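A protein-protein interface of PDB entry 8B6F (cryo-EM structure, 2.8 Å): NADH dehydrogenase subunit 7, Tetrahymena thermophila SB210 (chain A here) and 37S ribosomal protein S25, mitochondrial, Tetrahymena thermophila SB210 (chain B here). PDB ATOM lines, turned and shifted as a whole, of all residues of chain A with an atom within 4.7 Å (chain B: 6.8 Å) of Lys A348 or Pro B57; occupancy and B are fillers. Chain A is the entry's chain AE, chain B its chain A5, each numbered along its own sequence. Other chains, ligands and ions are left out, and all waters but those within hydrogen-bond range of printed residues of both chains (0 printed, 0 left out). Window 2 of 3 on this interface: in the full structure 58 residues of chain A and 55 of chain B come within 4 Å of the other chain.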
ATOM      1  N   ASN A 343      25.228  26.160 -34.015  1.00  0.00           N
ATOM      2  CA  ASN A 343      25.987  25.212 -33.204  1.00  0.00           C
ATOM      3  C   ASN A 343      25.401  25.092 -31.803  1.00  0.00           C
ATOM      4  O   ASN A 343      25.260  23.983 -31.274  1.00  0.00           O
ATOM      5  CB  ASN A 343      27.452  25.639 -33.130  1.00  0.00           C
ATOM      6  CG  ASN A 343      28.160  25.508 -34.458  1.00  0.00           C
ATOM      7  OD1 ASN A 343      27.793  24.679 -35.288  1.00  0.00           O
ATOM      8  ND2 ASN A 343      29.186  26.324 -34.665  1.00  0.00           N
ATOM      9  N   LEU A 344      25.065  26.221 -31.181  1.00  0.00           N
ATOM     10  CA  LEU A 344      24.469  26.180 -29.851  1.00  0.00           C
ATOM     11  C   LEU A 344      23.131  25.454 -29.875  1.00  0.00           C
ATOM     12  O   LEU A 344      22.837  24.644 -28.989  1.00  0.00           O
ATOM     13  CB  LEU A 344      24.303  27.597 -29.307  1.00  0.00           C
ATOM     14  CG  LEU A 344      25.602  28.361 -29.045  1.00  0.00           C
ATOM     15  CD1 LEU A 344      25.306  29.819 -28.749  1.00  0.00           C
ATOM     16  CD2 LEU A 344      26.375  27.730 -27.902  1.00  0.00           C
ATOM     17  N   LYS A 345      22.305  25.737 -30.884  1.00  0.00           N
ATOM     18  CA  LYS A 345      20.999  25.094 -30.977  1.00  0.00           C
ATOM     19  C   LYS A 345      21.133  23.582 -31.104  1.00  0.00           C
ATOM     20  O   LYS A 345      20.387  22.829 -30.466  1.00  0.00           O
ATOM     21  CB  LYS A 345      20.233  25.669 -32.170  1.00  0.00           C
ATOM     22  CG  LYS A 345      18.811  25.154 -32.328  1.00  0.00           C
ATOM     23  CD  LYS A 345      17.880  25.743 -31.281  1.00  0.00           C
ATOM     24  CE  LYS A 345      16.436  25.347 -31.550  1.00  0.00           C
ATOM     25  NZ  LYS A 345      15.500  25.974 -30.576  1.00  0.00           N
ATOM     26  N   ASN A 346      22.074  23.116 -31.921  1.00  0.00           N
ATOM     27  CA  ASN A 346      22.220  21.693 -32.190  1.00  0.00           C
ATOM     28  C   ASN A 346      23.100  20.965 -31.183  1.00  0.00           C
ATOM     29  O   ASN A 346      23.158  19.732 -31.223  1.00  0.00           O
ATOM     30  CB  ASN A 346      22.790  21.486 -33.597  1.00  0.00           C
ATOM     31  CG  ASN A 346      21.833  21.937 -34.680  1.00  0.00           C
ATOM     32  OD1 ASN A 346      20.974  21.177 -35.120  1.00  0.00           O
ATOM     33  ND2 ASN A 346      21.974  23.183 -35.112  1.00  0.00           N
ATOM     34  N   THR A 347      23.782  21.679 -30.288  1.00  0.00           N
ATOM     35  CA  THR A 347      24.639  21.040 -29.298  1.00  0.00           C
ATOM     36  C   THR A 347      24.089  21.085 -27.882  1.00  0.00           C
ATOM     37  O   THR A 347      24.313  20.142 -27.122  1.00  0.00           O
ATOM     38  CB  THR A 347      26.029  21.693 -29.298  1.00  0.00           C
ATOM     39  OG1 THR A 347      26.562  21.695 -30.628  1.00  0.00           O
ATOM     40  CG2 THR A 347      26.982  20.937 -28.382  1.00  0.00           C
ATOM     41  N   LYS A 348      23.384  22.147 -27.503  1.00  0.00           N
ATOM     42  CA  LYS A 348      22.878  22.312 -26.148  1.00  0.00           C
ATOM     43  C   LYS A 348      21.372  22.094 -26.127  1.00  0.00           C
ATOM     44  O   LYS A 348      20.640  22.715 -26.903  1.00  0.00           O
ATOM     45  CB  LYS A 348      23.215  23.703 -25.602  1.00  0.00           C
ATOM     46  CG  LYS A 348      24.593  23.805 -24.964  1.00  0.00           C
ATOM     47  CD  LYS A 348      25.704  23.644 -25.987  1.00  0.00           C
ATOM     48  CE  LYS A 348      27.075  23.741 -25.336  1.00  0.00           C
ATOM     49  NZ  LYS A 348      27.294  22.668 -24.327  1.00  0.00           N
ATOM     50  N   ASN A 349      20.918  21.215 -25.238  1.00  0.00           N
ATOM     51  CA  ASN A 349      19.499  20.970 -25.031  1.00  0.00           C
ATOM     52  C   ASN A 349      19.246  20.870 -23.532  1.00  0.00           C
ATOM     53  O   ASN A 349      20.148  21.067 -22.714  1.00  0.00           O
ATOM     54  CB  ASN A 349      19.037  19.716 -25.782  1.00  0.00           C
ATOM     55  CG  ASN A 349      19.884  18.506 -25.469  1.00  0.00           C
ATOM     56  OD1 ASN A 349      19.631  17.790 -24.505  1.00  0.00           O
ATOM     57  ND2 ASN A 349      20.897  18.266 -26.293  1.00  0.00           N
ATOM     58  N   ASN A 352      21.233  18.170 -21.042  1.00  0.00           N
ATOM     59  CA  ASN A 352      22.645  18.274 -20.691  1.00  0.00           C
ATOM     60  C   ASN A 352      23.087  19.662 -20.259  1.00  0.00           C
ATOM     61  O   ASN A 352      24.210  19.791 -19.763  1.00  0.00           O
ATOM     62  CB  ASN A 352      23.520  17.824 -21.870  1.00  0.00           C
ATOM     63  CG  ASN A 352      23.250  18.614 -23.133  1.00  0.00           C
ATOM     64  OD1 ASN A 352      22.717  19.721 -23.086  1.00  0.00           O
ATOM     65  ND2 ASN A 352      23.617  18.044 -24.274  1.00  0.00           N
ATOM     66  N   SER A 353      22.270  20.699 -20.425  1.00  0.00           N
ATOM     67  CA  SER A 353      22.637  22.061 -20.061  1.00  0.00           C
ATOM     68  C   SER A 353      21.670  22.587 -19.009  1.00  0.00           C
ATOM     69  O   SER A 353      20.452  22.542 -19.202  1.00  0.00           O
ATOM     70  CB  SER A 353      22.637  22.971 -21.292  1.00  0.00           C
ATOM     71  OG  SER A 353      22.959  24.305 -20.943  1.00  0.00           O
ATOM     72  N   GLU A 356      19.661  25.531 -20.389  1.00  0.00           N
ATOM     73  CA  GLU A 356      18.615  25.063 -21.291  1.00  0.00           C
ATOM     74  C   GLU A 356      17.458  24.450 -20.514  1.00  0.00           C
ATOM     75  O   GLU A 356      16.290  24.669 -20.851  1.00  0.00           O
ATOM     76  CB  GLU A 356      19.186  24.046 -22.278  1.00  0.00           C
ATOM     77  CG  GLU A 356      20.184  24.629 -23.262  1.00  0.00           C
ATOM     78  CD  GLU A 356      19.527  25.524 -24.295  1.00  0.00           C
ATOM     79  OE1 GLU A 356      18.295  25.711 -24.224  1.00  0.00           O
ATOM     80  OE2 GLU A 356      20.243  26.035 -25.181  1.00  0.00           O
ATOM     81  N   ILE B  47      30.799  19.193 -36.431  1.00  0.00           N
ATOM     82  CA  ILE B  47      31.614  20.340 -36.049  1.00  0.00           C
ATOM     83  C   ILE B  47      33.064  19.886 -35.987  1.00  0.00           C
ATOM     84  O   ILE B  47      33.362  18.825 -35.426  1.00  0.00           O
ATOM     85  CB  ILE B  47      31.176  20.933 -34.695  1.00  0.00           C
ATOM     86  CG1 ILE B  47      29.688  21.292 -34.730  1.00  0.00           C
ATOM     87  CG2 ILE B  47      32.017  22.159 -34.360  1.00  0.00           C
ATOM     88  CD1 ILE B  47      29.133  21.773 -33.404  1.00  0.00           C
ATOM     89  N   THR B  51      37.048  24.892 -35.577  1.00  0.00           N
ATOM     90  CA  THR B  51      36.049  25.948 -35.639  1.00  0.00           C
ATOM     91  C   THR B  51      36.453  27.107 -34.738  1.00  0.00           C
ATOM     92  O   THR B  51      36.908  26.910 -33.608  1.00  0.00           O
ATOM     93  CB  THR B  51      34.681  25.409 -35.220  1.00  0.00           C
ATOM     94  OG1 THR B  51      34.352  24.259 -36.009  1.00  0.00           O
ATOM     95  CG2 THR B  51      33.604  26.468 -35.411  1.00  0.00           C
ATOM     96  N   ALA B  52      36.280  28.324 -35.246  1.00  0.00           N
ATOM     97  CA  ALA B  52      36.673  29.509 -34.501  1.00  0.00           C
ATOM     98  C   ALA B  52      35.830  29.648 -33.240  1.00  0.00           C
ATOM     99  O   ALA B  52      34.680  29.209 -33.181  1.00  0.00           O
ATOM    100  CB  ALA B  52      36.526  30.756 -35.372  1.00  0.00           C
ATOM    101  N   PHE B  53      36.419  30.271 -32.217  1.00  0.00           N
ATOM    102  CA  PHE B  53      35.710  30.439 -30.954  1.00  0.00           C
ATOM    103  C   PHE B  53      34.436  31.248 -31.146  1.00  0.00           C
ATOM    104  O   PHE B  53      33.387  30.909 -30.587  1.00  0.00           O
ATOM    105  CB  PHE B  53      36.625  31.110 -29.930  1.00  0.00           C
ATOM    106  CG  PHE B  53      35.933  31.482 -28.651  1.00  0.00           C
ATOM    107  CD1 PHE B  53      35.681  30.528 -27.682  1.00  0.00           C
ATOM    108  CD2 PHE B  53      35.548  32.790 -28.413  1.00  0.00           C
ATOM    109  CE1 PHE B  53      35.048  30.869 -26.503  1.00  0.00           C
ATOM    110  CE2 PHE B  53      34.916  33.138 -27.238  1.00  0.00           C
ATOM    111  CZ  PHE B  53      34.666  32.177 -26.281  1.00  0.00           C
ATOM    112  N   ASP B  55      32.514  31.216 -33.496  1.00  0.00           N
ATOM    113  CA  ASP B  55      31.516  30.372 -34.136  1.00  0.00           C
ATOM    114  C   ASP B  55      31.299  29.043 -33.430  1.00  0.00           C
ATOM    115  O   ASP B  55      30.382  28.306 -33.806  1.00  0.00           O
ATOM    116  CB  ASP B  55      31.914  30.095 -35.593  1.00  0.00           C
ATOM    117  CG  ASP B  55      32.029  31.359 -36.416  1.00  0.00           C
ATOM    118  OD1 ASP B  55      31.657  32.435 -35.907  1.00  0.00           O
ATOM    119  OD2 ASP B  55      32.495  31.276 -37.571  1.00  0.00           O
ATOM    120  N   SER B  56      32.107  28.717 -32.430  1.00  0.00           N
ATOM    121  CA  SER B  56      32.049  27.422 -31.771  1.00  0.00           C
ATOM    122  C   SER B  56      30.897  27.367 -30.780  1.00  0.00           C
ATOM    123  O   SER B  56      30.323  28.392 -30.409  1.00  0.00           O
ATOM    124  CB  SER B  56      33.349  27.167 -31.025  1.00  0.00           C
ATOM    125  OG  SER B  56      33.441  28.087 -29.954  1.00  0.00           O
ATOM    126  N   PRO B  57      30.527  26.165 -30.326  1.00  0.00           N
ATOM    127  CA  PRO B  57      29.502  26.057 -29.276  1.00  0.00           C
ATOM    128  C   PRO B  57      29.953  26.578 -27.920  1.00  0.00           C
ATOM    129  O   PRO B  57      29.158  26.550 -26.974  1.00  0.00           O
ATOM    130  CB  PRO B  57      29.226  24.544 -29.206  1.00  0.00           C
ATOM    131  CG  PRO B  57      29.854  23.953 -30.421  1.00  0.00           C
ATOM    132  CD  PRO B  57      30.988  24.844 -30.782  1.00  0.00           C
ATOM    133  N   HIS B  58      31.196  27.041 -27.789  1.00  0.00           N
ATOM    134  CA  HIS B  58      31.736  27.516 -26.521  1.00  0.00           C
ATOM    135  C   HIS B  58      31.640  29.027 -26.368  1.00  0.00           C
ATOM    136  O   HIS B  58      32.257  29.585 -25.457  1.00  0.00           O
ATOM    137  CB  HIS B  58      33.196  27.080 -26.376  1.00  0.00           C
ATOM    138  CG  HIS B  58      33.409  25.611 -26.559  1.00  0.00           C
ATOM    139  ND1 HIS B  58      33.198  24.696 -25.549  1.00  0.00           N
ATOM    140  CD2 HIS B  58      33.820  24.897 -27.633  1.00  0.00           C
ATOM    141  CE1 HIS B  58      33.466  23.482 -25.995  1.00  0.00           C
ATOM    142  NE2 HIS B  58      33.846  23.577 -27.257  1.00  0.00           N
ATOM    143  N   ASN B  59      30.899  29.700 -27.239  1.00  0.00           N
ATOM    144  CA  ASN B  59      30.725  31.149 -27.187  1.00  0.00           C
ATOM    145  C   ASN B  59      29.272  31.431 -26.813  1.00  0.00           C
ATOM    146  O   ASN B  59      28.409  31.570 -27.679  1.00  0.00           O
ATOM    147  CB  ASN B  59      31.098  31.788 -28.518  1.00  0.00           C
ATOM    148  CG  ASN B  59      30.972  33.294 -28.495  1.00  0.00           C
ATOM    149  OD1 ASN B  59      31.107  33.922 -27.446  1.00  0.00           O
ATOM    150  ND2 ASN B  59      30.709  33.883 -29.654  1.00  0.00           N
ATOM    151  N   ILE B  60      29.008  31.516 -25.507  1.00  0.00           N
ATOM    152  CA  ILE B  60      27.655  31.788 -25.036  1.00  0.00           C
ATOM    153  C   ILE B  60      27.409  33.271 -24.785  1.00  0.00           C
ATOM    154  O   ILE B  60      26.248  33.704 -24.790  1.00  0.00           O
ATOM    155  CB  ILE B  60      27.332  30.967 -23.770  1.00  0.00           C
ATOM    156  CG1 ILE B  60      28.325  31.205 -22.621  1.00  0.00           C
ATOM    157  CG2 ILE B  60      27.286  29.488 -24.104  1.00  0.00           C
ATOM    158  CD1 ILE B  60      28.134  32.485 -21.839  1.00  0.00           C
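ND2 of Asn A343 is in hydrogen-bond range of O of Asp B55, 2.5 Å away.
The backbone carbonyl oxygen (O) of Asn A343 sits at hydrogen-bond distance from the side-chain hydroxyl (OG1) of Thr A347.
Asn A343 touches Ile B47. CG of Pro B57 touches CB of Asn A343 (3.99 Å). Leu A344 touches Pro B57 (CD2 to O, 3.2 Å). O of Asn B59 touches CD1 of Leu A344 (3.7 Å). Thr A347 touches Ile B47 (OG1 to CD1, 3.8 Å). CG of Pro B57 touches OG1 of Thr A347, at 3.997 Å. CE of Lys A348 touches O of Pro B57 (3.9 Å).
Printed residues of chain A within 4 Å of Pro B57: Asn A343 (3.99 Å), Leu A344 (3.2 Å), Thr A347 (3.997 Å) and Lys A348 (3.9 Å). Of the printed residues of chain A, Asp B55 touches Asn A343. Of the printed residues of chain B, Thr A347 touches Ile B47 (3.8 Å) and Pro B57 (3.997 Å). Ser B56 touches none of the printed residues of chain A. The nearest residue of chain B that does not touch Lys A348 is His B58 (5.8 Å).
Hydrophobic or aromatic side chains of chain B within 4 Å of the printed part of chain A: Ile B47 and Pro B57. Hydrophobic or aromatic side chains of chain A within 4 Å of the printed part of chain B: Leu A344. Among the printed residues, no Asp or Glu carboxylate lies within 4 Å of a Lys or Arg side-chain nitrogen of the other chain.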
